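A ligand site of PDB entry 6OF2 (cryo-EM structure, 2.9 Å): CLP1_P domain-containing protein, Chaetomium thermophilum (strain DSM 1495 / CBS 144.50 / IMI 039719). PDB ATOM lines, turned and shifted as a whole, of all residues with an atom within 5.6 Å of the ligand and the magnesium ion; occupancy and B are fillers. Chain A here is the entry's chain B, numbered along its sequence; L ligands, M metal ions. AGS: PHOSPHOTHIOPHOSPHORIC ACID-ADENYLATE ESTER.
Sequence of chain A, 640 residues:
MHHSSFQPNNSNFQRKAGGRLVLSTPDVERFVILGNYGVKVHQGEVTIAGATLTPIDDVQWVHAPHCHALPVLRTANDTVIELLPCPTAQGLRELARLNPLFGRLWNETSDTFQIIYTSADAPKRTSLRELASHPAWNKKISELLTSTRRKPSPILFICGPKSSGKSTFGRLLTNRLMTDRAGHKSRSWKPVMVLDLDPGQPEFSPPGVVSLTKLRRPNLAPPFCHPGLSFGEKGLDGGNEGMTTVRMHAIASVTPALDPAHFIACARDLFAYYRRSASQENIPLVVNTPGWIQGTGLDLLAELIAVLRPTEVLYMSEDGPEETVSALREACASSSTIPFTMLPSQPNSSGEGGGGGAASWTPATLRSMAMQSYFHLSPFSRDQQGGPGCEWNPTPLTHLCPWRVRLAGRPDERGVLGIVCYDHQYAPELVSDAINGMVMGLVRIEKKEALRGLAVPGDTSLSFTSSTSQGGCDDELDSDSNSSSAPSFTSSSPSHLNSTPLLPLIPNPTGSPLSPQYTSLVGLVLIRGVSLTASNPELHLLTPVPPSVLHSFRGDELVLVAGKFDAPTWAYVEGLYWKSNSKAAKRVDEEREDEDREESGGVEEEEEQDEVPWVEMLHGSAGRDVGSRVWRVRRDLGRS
CB of Ala 69 touches N3 of the ligand (3.9 Å). Glu 130 touches the ligand. CA of Leu 131 touches C2 of the ligand, 3.5 Å away. Ser 133 touches the ligand (N to N6, 3.99 Å). Lys 162 touches the ligand (CA to O2G, 3.7 Å). Lys 166 touches the ligand (CE to O1B, 3.1 Å). OE1 of Gln 201 touches S1G of the ligand, 3.9 Å away. Ser 345 touches the ligand (O to N7, 3.9 Å). Hydrophobic or aromatic side chains that line the ligand: Ala 69 and Leu 131. The nearest printed residue that does not touch the ligand is Trp 137 (4.1 Å).
The magnesium ion is bound by O3G of the ligand, 2.1 Å away. OG of Ser 167 binds the magnesium ion, 2.1 Å away. The magnesium ion is bound by O2B of the ligand, at 2.1 Å. The magnesium ion has three donor atoms within binding distance.
An oxygen (O3A) of the ligand is in hydrogen-bond range of the backbone NH (N) of Gly 165 (3.3 Å). N6 of the ligand lies within hydrogen-bond range of OE1 of Gln 346. N of Ser 164 lies within hydrogen-bond range of O1B of the ligand (3.3 Å). O1A of the ligand is in hydrogen-bond range of N of Thr 168. The side-chain hydroxyl of Thr 168 sits at hydrogen-bond distance from an oxygen (O1A) of the ligand. The backbone carbonyl oxygen of Ala 132 sits at hydrogen-bond distance from a nitrogen (N6) of the ligand (2.9 Å). N1 of the ligand lies within hydrogen-bond range of N of Ala 132, at 2.9 Å. The backbone NH of Ser 163 lies within hydrogen-bond range of an oxygen (O2G) of the ligand, 3.4 Å away. The guanidinium group (NH1) of Arg 129 lies within hydrogen-bond range of an oxygen (O3') of the ligand (2.9 Å). O1A of the ligand sits at hydrogen-bond distance from N of Ser 167.
The side-chain amide nitrogen of Gln 346 sits close to the backbone NH of His 134 (3.3 Å). N of Gln 201 is in hydrogen-bond range of OD1 of Asp 198 (2.8 Å).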
ATOM      1  N   HIS A  68      14.478   4.639  26.492  1.00  0.00           N
ATOM      2  CA  HIS A  68      14.520   3.202  26.720  1.00  0.00           C
ATOM      3  C   HIS A  68      15.667   2.791  27.625  1.00  0.00           C
ATOM      4  O   HIS A  68      16.151   3.594  28.428  1.00  0.00           O
ATOM      5  CB  HIS A  68      14.624   2.457  25.388  1.00  0.00           C
ATOM      6  CG  HIS A  68      13.457   2.684  24.477  1.00  0.00           C
ATOM      7  ND1 HIS A  68      13.051   3.928  24.072  1.00  0.00           N
ATOM      8  CD2 HIS A  68      12.606   1.807  23.892  1.00  0.00           C
ATOM      9  CE1 HIS A  68      12.006   3.821  23.280  1.00  0.00           C
ATOM     10  NE2 HIS A  68      11.717   2.543  23.156  1.00  0.00           N
ATOM     11  N   ALA A  69      16.114   1.547  27.493  1.00  0.00           N
ATOM     12  CA  ALA A  69      17.207   1.023  28.303  1.00  0.00           C
ATOM     13  C   ALA A  69      18.493   1.094  27.496  1.00  0.00           C
ATOM     14  O   ALA A  69      18.632   0.407  26.488  1.00  0.00           O
ATOM     15  CB  ALA A  69      16.911  -0.416  28.745  1.00  0.00           C
ATOM     16  N   ARG A 129      17.489   3.874  33.345  1.00  0.00           N
ATOM     17  CA  ARG A 129      17.349   2.426  33.411  1.00  0.00           C
ATOM     18  C   ARG A 129      18.593   1.785  32.797  1.00  0.00           C
ATOM     19  O   ARG A 129      19.579   2.453  32.470  1.00  0.00           O
ATOM     20  CB  ARG A 129      16.084   1.984  32.682  1.00  0.00           C
ATOM     21  CG  ARG A 129      14.826   2.686  33.128  1.00  0.00           C
ATOM     22  CD  ARG A 129      13.674   2.316  32.205  1.00  0.00           C
ATOM     23  NE  ARG A 129      12.469   3.086  32.494  1.00  0.00           N
ATOM     24  CZ  ARG A 129      11.344   2.973  31.800  1.00  0.00           C
ATOM     25  NH1 ARG A 129      11.270   2.131  30.782  1.00  0.00           N
ATOM     26  NH2 ARG A 129      10.288   3.713  32.119  1.00  0.00           N
ATOM     27  N   GLU A 130      18.555   0.471  32.638  1.00  0.00           N
ATOM     28  CA  GLU A 130      19.670  -0.250  32.039  1.00  0.00           C
ATOM     29  C   GLU A 130      19.174  -1.581  31.505  1.00  0.00           C
ATOM     30  O   GLU A 130      18.354  -2.239  32.154  1.00  0.00           O
ATOM     31  CB  GLU A 130      20.801  -0.458  33.044  1.00  0.00           C
ATOM     32  CG  GLU A 130      21.972  -1.222  32.493  1.00  0.00           C
ATOM     33  CD  GLU A 130      23.046  -1.453  33.538  1.00  0.00           C
ATOM     34  OE1 GLU A 130      23.635  -0.454  34.011  1.00  0.00           O
ATOM     35  OE2 GLU A 130      23.304  -2.617  33.880  1.00  0.00           O
ATOM     36  N   LEU A 131      19.675  -1.979  30.338  1.00  0.00           N
ATOM     37  CA  LEU A 131      19.277  -3.236  29.719  1.00  0.00           C
ATOM     38  C   LEU A 131      19.860  -4.416  30.470  1.00  0.00           C
ATOM     39  O   LEU A 131      21.091  -4.589  30.503  1.00  0.00           O
ATOM     40  CB  LEU A 131      19.707  -3.254  28.254  1.00  0.00           C
ATOM     41  CG  LEU A 131      19.295  -4.476  27.446  1.00  0.00           C
ATOM     42  CD1 LEU A 131      17.789  -4.530  27.280  1.00  0.00           C
ATOM     43  CD2 LEU A 131      19.976  -4.481  26.100  1.00  0.00           C
ATOM     44  N   ALA A 132      19.011  -5.242  31.062  1.00  0.00           N
ATOM     45  CA  ALA A 132      19.438  -6.440  31.769  1.00  0.00           C
ATOM     46  C   ALA A 132      18.802  -7.657  31.093  1.00  0.00           C
ATOM     47  O   ALA A 132      18.146  -7.538  30.050  1.00  0.00           O
ATOM     48  CB  ALA A 132      19.075  -6.362  33.251  1.00  0.00           C
ATOM     49  N   SER A 133      18.967  -8.832  31.703  1.00  0.00           N
ATOM     50  CA  SER A 133      18.420 -10.050  31.132  1.00  0.00           C
ATOM     51  C   SER A 133      18.561 -11.265  32.040  1.00  0.00           C
ATOM     52  O   SER A 133      19.675 -11.612  32.443  1.00  0.00           O
ATOM     53  CB  SER A 133      19.109 -10.374  29.797  1.00  0.00           C
ATOM     54  OG  SER A 133      20.482 -10.616  29.999  1.00  0.00           O
ATOM     55  N   HIS A 134      17.442 -11.903  32.364  1.00  0.00           N
ATOM     56  CA  HIS A 134      17.503 -13.117  33.162  1.00  0.00           C
ATOM     57  C   HIS A 134      18.323 -14.167  32.429  1.00  0.00           C
ATOM     58  O   HIS A 134      18.310 -14.221  31.197  1.00  0.00           O
ATOM     59  CB  HIS A 134      16.099 -13.672  33.413  1.00  0.00           C
ATOM     60  CG  HIS A 134      15.359 -12.991  34.517  1.00  0.00           C
ATOM     61  ND1 HIS A 134      15.817 -12.957  35.818  1.00  0.00           N
ATOM     62  CD2 HIS A 134      14.172 -12.342  34.524  1.00  0.00           C
ATOM     63  CE1 HIS A 134      14.958 -12.297  36.579  1.00  0.00           C
ATOM     64  NE2 HIS A 134      13.947 -11.913  35.813  1.00  0.00           N
ATOM     65  N   TRP A 137      16.392 -16.183  29.652  1.00  0.00           N
ATOM     66  CA  TRP A 137      16.292 -15.598  28.318  1.00  0.00           C
ATOM     67  C   TRP A 137      17.479 -16.002  27.457  1.00  0.00           C
ATOM     68  O   TRP A 137      17.312 -16.521  26.346  1.00  0.00           O
ATOM     69  CB  TRP A 137      16.234 -14.078  28.430  1.00  0.00           C
ATOM     70  CG  TRP A 137      14.894 -13.524  28.735  1.00  0.00           C
ATOM     71  CD1 TRP A 137      13.866 -14.170  29.335  1.00  0.00           C
ATOM     72  CD2 TRP A 137      14.451 -12.187  28.502  1.00  0.00           C
ATOM     73  NE1 TRP A 137      12.796 -13.321  29.468  1.00  0.00           N
ATOM     74  CE2 TRP A 137      13.133 -12.102  28.966  1.00  0.00           C
ATOM     75  CE3 TRP A 137      15.040 -11.066  27.926  1.00  0.00           C
ATOM     76  CZ2 TRP A 137      12.390 -10.934  28.885  1.00  0.00           C
ATOM     77  CZ3 TRP A 137      14.302  -9.901  27.853  1.00  0.00           C
ATOM     78  CH2 TRP A 137      12.990  -9.850  28.325  1.00  0.00           C
ATOM     79  N   PRO A 161       1.350 -10.624  27.188  1.00  0.00           N
ATOM     80  CA  PRO A 161       0.624  -9.456  27.682  1.00  0.00           C
ATOM     81  C   PRO A 161       1.409  -8.163  27.543  1.00  0.00           C
ATOM     82  O   PRO A 161       2.625  -8.155  27.355  1.00  0.00           O
ATOM     83  CB  PRO A 161       0.370  -9.807  29.143  1.00  0.00           C
ATOM     84  CG  PRO A 161       1.558 -10.620  29.485  1.00  0.00           C
ATOM     85  CD  PRO A 161       1.689 -11.527  28.299  1.00  0.00           C
ATOM     86  N   LYS A 162       0.679  -7.055  27.631  1.00  0.00           N
ATOM     87  CA  LYS A 162       1.274  -5.724  27.529  1.00  0.00           C
ATOM     88  C   LYS A 162       2.413  -5.564  28.531  1.00  0.00           C
ATOM     89  O   LYS A 162       2.363  -6.087  29.647  1.00  0.00           O
ATOM     90  CB  LYS A 162       0.234  -4.641  27.780  1.00  0.00           C
ATOM     91  CG  LYS A 162      -0.770  -4.470  26.655  1.00  0.00           C
ATOM     92  CD  LYS A 162      -1.559  -3.185  26.848  1.00  0.00           C
ATOM     93  CE  LYS A 162      -2.479  -2.938  25.673  1.00  0.00           C
ATOM     94  NZ  LYS A 162      -3.242  -1.668  25.830  1.00  0.00           N
ATOM     95  N   SER A 163       3.426  -4.803  28.121  1.00  0.00           N
ATOM     96  CA  SER A 163       4.602  -4.507  28.926  1.00  0.00           C
ATOM     97  C   SER A 163       5.184  -5.779  29.555  1.00  0.00           C
ATOM     98  O   SER A 163       5.288  -5.911  30.771  1.00  0.00           O
ATOM     99  CB  SER A 163       4.286  -3.467  29.993  1.00  0.00           C
ATOM    100  OG  SER A 163       3.861  -2.251  29.404  1.00  0.00           O
ATOM    101  N   SER A 164       5.546  -6.708  28.700  1.00  0.00           N
ATOM    102  CA  SER A 164       6.113  -7.979  29.116  1.00  0.00           C
ATOM    103  C   SER A 164       7.532  -8.200  28.636  1.00  0.00           C
ATOM    104  O   SER A 164       8.288  -8.905  29.294  1.00  0.00           O
ATOM    105  CB  SER A 164       5.242  -9.145  28.634  1.00  0.00           C
ATOM    106  OG  SER A 164       5.818 -10.374  29.011  1.00  0.00           O
ATOM    107  N   GLY A 165       7.911  -7.624  27.503  1.00  0.00           N
ATOM    108  CA  GLY A 165       9.247  -7.781  26.989  1.00  0.00           C
ATOM    109  C   GLY A 165       9.291  -8.425  25.622  1.00  0.00           C
ATOM    110  O   GLY A 165      10.347  -8.928  25.206  1.00  0.00           O
ATOM    111  N   LYS A 166       8.157  -8.441  24.921  1.00  0.00           N
ATOM    112  CA  LYS A 166       8.121  -9.017  23.581  1.00  0.00           C
ATOM    113  C   LYS A 166       9.115  -8.308  22.666  1.00  0.00           C
ATOM    114  O   LYS A 166       9.934  -8.950  22.013  1.00  0.00           O
ATOM    115  CB  LYS A 166       6.710  -8.926  23.010  1.00  0.00           C
ATOM    116  CG  LYS A 166       5.668  -9.700  23.769  1.00  0.00           C
ATOM    117  CD  LYS A 166       4.286  -9.311  23.317  1.00  0.00           C
ATOM    118  CE  LYS A 166       4.032  -7.850  23.583  1.00  0.00           C
ATOM    119  NZ  LYS A 166       2.658  -7.436  23.222  1.00  0.00           N
ATOM    120  N   SER A 167       9.041  -6.984  22.627  1.00  0.00           N
ATOM    121  CA  SER A 167       9.916  -6.206  21.752  1.00  0.00           C
ATOM    122  C   SER A 167      11.386  -6.417  22.091  1.00  0.00           C
ATOM    123  O   SER A 167      12.190  -6.765  21.222  1.00  0.00           O
ATOM    124  CB  SER A 167       9.554  -4.723  21.846  1.00  0.00           C
ATOM    125  OG  SER A 167       8.248  -4.486  21.337  1.00  0.00           O
ATOM    126  N   THR A 168      11.764  -6.161  23.353  1.00  0.00           N
ATOM    127  CA  THR A 168      13.156  -6.328  23.758  1.00  0.00           C
ATOM    128  C   THR A 168      13.677  -7.710  23.414  1.00  0.00           C
ATOM    129  O   THR A 168      14.786  -7.866  22.896  1.00  0.00           O
ATOM    130  CB  THR A 168      13.286  -6.049  25.249  1.00  0.00           C
ATOM    131  OG1 THR A 168      12.907  -4.697  25.516  1.00  0.00           O
ATOM    132  CG2 THR A 168      14.727  -6.249  25.673  1.00  0.00           C
ATOM    133  N   PHE A 169      12.897  -8.744  23.746  1.00  0.00           N
ATOM    134  CA  PHE A 169      13.324 -10.098  23.424  1.00  0.00           C
ATOM    135  C   PHE A 169      13.556 -10.250  21.935  1.00  0.00           C
ATOM    136  O   PHE A 169      14.552 -10.837  21.513  1.00  0.00           O
ATOM    137  CB  PHE A 169      12.293 -11.114  23.923  1.00  0.00           C
ATOM    138  CG  PHE A 169      12.743 -12.518  23.765  1.00  0.00           C
ATOM    139  CD1 PHE A 169      13.962 -12.932  24.275  1.00  0.00           C
ATOM    140  CD2 PHE A 169      11.961 -13.440  23.120  1.00  0.00           C
ATOM    141  CE1 PHE A 169      14.377 -14.224  24.145  1.00  0.00           C
ATOM    142  CE2 PHE A 169      12.375 -14.742  22.987  1.00  0.00           C
ATOM    143  CZ  PHE A 169      13.591 -15.133  23.494  1.00  0.00           C
ATOM    144  N   ASP A 198       2.026  -5.172  14.357  1.00  0.00           N
ATOM    145  CA  ASP A 198       1.559  -4.421  15.524  1.00  0.00           C
ATOM    146  C   ASP A 198       1.299  -2.982  15.137  1.00  0.00           C
ATOM    147  O   ASP A 198       2.214  -2.147  15.142  1.00  0.00           O
ATOM    148  CB  ASP A 198       2.577  -4.513  16.657  1.00  0.00           C
ATOM    149  CG  ASP A 198       2.115  -3.823  17.922  1.00  0.00           C
ATOM    150  OD1 ASP A 198       1.914  -2.587  17.920  1.00  0.00           O
ATOM    151  OD2 ASP A 198       1.945  -4.524  18.949  1.00  0.00           O
ATOM    152  N   GLN A 201       2.333   0.162  18.453  1.00  0.00           N
ATOM    153  CA  GLN A 201       3.669   0.732  18.549  1.00  0.00           C
ATOM    154  C   GLN A 201       4.531  -0.072  17.595  1.00  0.00           C
ATOM    155  O   GLN A 201       5.216  -1.028  17.992  1.00  0.00           O
ATOM    156  CB  GLN A 201       4.199   0.667  19.979  1.00  0.00           C
ATOM    157  CG  GLN A 201       5.520   1.385  20.191  1.00  0.00           C
ATOM    158  CD  GLN A 201       5.970   1.330  21.626  1.00  0.00           C
ATOM    159  OE1 GLN A 201       5.249   1.727  22.535  1.00  0.00           O
ATOM    160  NE2 GLN A 201       7.186   0.832  21.844  1.00  0.00           N
ATOM    161  N   GLY A 291      -0.621  -6.913  21.629  1.00  0.00           N
ATOM    162  CA  GLY A 291      -0.606  -7.167  23.055  1.00  0.00           C
ATOM    163  C   GLY A 291      -1.963  -7.488  23.639  1.00  0.00           C
ATOM    164  O   GLY A 291      -2.274  -7.097  24.770  1.00  0.00           O
ATOM    165  N   SER A 345       9.084 -12.012  32.706  1.00  0.00           N
ATOM    166  CA  SER A 345       8.718 -10.753  32.083  1.00  0.00           C
ATOM    167  C   SER A 345       9.529  -9.557  32.564  1.00  0.00           C
ATOM    168  O   SER A 345       9.775  -8.624  31.787  1.00  0.00           O
ATOM    169  CB  SER A 345       7.236 -10.472  32.314  1.00  0.00           C
ATOM    170  OG  SER A 345       6.931 -10.458  33.696  1.00  0.00           O
ATOM    171  N   GLN A 346       9.913  -9.547  33.841  1.00  0.00           N
ATOM    172  CA  GLN A 346      10.675  -8.433  34.410  1.00  0.00           C
ATOM    173  C   GLN A 346       9.867  -7.134  34.383  1.00  0.00           C
ATOM    174  O   GLN A 346      10.240  -6.197  33.677  1.00  0.00           O
ATOM    175  CB  GLN A 346      12.025  -8.225  33.713  1.00  0.00           C
ATOM    176  CG  GLN A 346      12.985  -9.364  33.878  1.00  0.00           C
ATOM    177  CD  GLN A 346      14.292  -9.141  33.152  1.00  0.00           C
ATOM    178  OE1 GLN A 346      14.971  -8.135  33.373  1.00  0.00           O
ATOM    179  NE2 GLN A 346      14.675 -10.082  32.291  1.00  0.00           N
ATOM    180  N   PRO A 363       2.570   4.757  25.962  1.00  0.00           N
ATOM    181  CA  PRO A 363       2.545   4.381  24.541  1.00  0.00           C
ATOM    182  C   PRO A 363       2.102   5.497  23.614  1.00  0.00           C
ATOM    183  O   PRO A 363       2.651   5.638  22.520  1.00  0.00           O
ATOM    184  CB  PRO A 363       1.569   3.199  24.532  1.00  0.00           C
ATOM    185  CG  PRO A 363       1.820   2.568  25.839  1.00  0.00           C
ATOM    186  CD  PRO A 363       1.866   3.742  26.776  1.00  0.00           C
HETATM  187  PG  AGS L   1       4.327  -3.118  24.508  1.00  0.00           P
HETATM  188  S1G AGS L   1       3.876  -1.232  24.636  1.00  0.00           S
HETATM  189  O2G AGS L   1       3.144  -3.992  24.809  1.00  0.00           O
HETATM  190  O3G AGS L   1       4.856  -3.463  23.144  1.00  0.00           O
HETATM  191  PB  AGS L   1       6.458  -4.766  25.140  1.00  0.00           P
HETATM  192  O1B AGS L   1       5.680  -5.994  25.521  1.00  0.00           O
HETATM  193  O2B AGS L   1       6.975  -4.624  23.729  1.00  0.00           O
HETATM  194  O3B AGS L   1       5.550  -3.486  25.481  1.00  0.00           O
HETATM  195  PA  AGS L   1       9.034  -3.934  25.651  1.00  0.00           P
HETATM  196  O1A AGS L   1       9.967  -5.011  25.172  1.00  0.00           O
HETATM  197  O2A AGS L   1       8.643  -2.807  24.732  1.00  0.00           O
HETATM  198  O3A AGS L   1       7.690  -4.634  26.158  1.00  0.00           O
HETATM  199  O5' AGS L   1       9.667  -3.268  26.967  1.00  0.00           O
HETATM  200  C5' AGS L   1       8.857  -2.534  27.886  1.00  0.00           C
HETATM  201  C4' AGS L   1       9.764  -1.879  28.886  1.00  0.00           C
HETATM  202  O4' AGS L   1      10.296  -2.865  29.793  1.00  0.00           O
HETATM  203  C3' AGS L   1      10.957  -1.142  28.290  1.00  0.00           C
HETATM  204  O3' AGS L   1      10.898   0.237  28.562  1.00  0.00           O
HETATM  205  C2' AGS L   1      12.192  -1.809  28.869  1.00  0.00           C
HETATM  206  O2' AGS L   1      13.062  -0.823  29.395  1.00  0.00           O
HETATM  207  C1' AGS L   1      11.648  -2.615  30.045  1.00  0.00           C
HETATM  208  N9  AGS L   1      12.330  -3.909  30.267  1.00  0.00           N
HETATM  209  C8  AGS L   1      11.732  -5.120  30.502  1.00  0.00           C
HETATM  210  N7  AGS L   1      12.577  -6.105  30.662  1.00  0.00           N
HETATM  211  C5  AGS L   1      13.815  -5.502  30.510  1.00  0.00           C
HETATM  212  C6  AGS L   1      15.111  -6.018  30.570  1.00  0.00           C
HETATM  213  N6  AGS L   1      15.397  -7.300  30.800  1.00  0.00           N
HETATM  214  N1  AGS L   1      16.142  -5.165  30.383  1.00  0.00           N
HETATM  215  C2  AGS L   1      15.856  -3.883  30.153  1.00  0.00           C
HETATM  216  N3  AGS L   1      14.669  -3.274  30.083  1.00  0.00           N
HETATM  217  C4  AGS L   1      13.684  -4.154  30.268  1.00  0.00           C
HETATM  218 MG    MG M   1       6.599  -3.458  22.044  1.00  0.00          MG
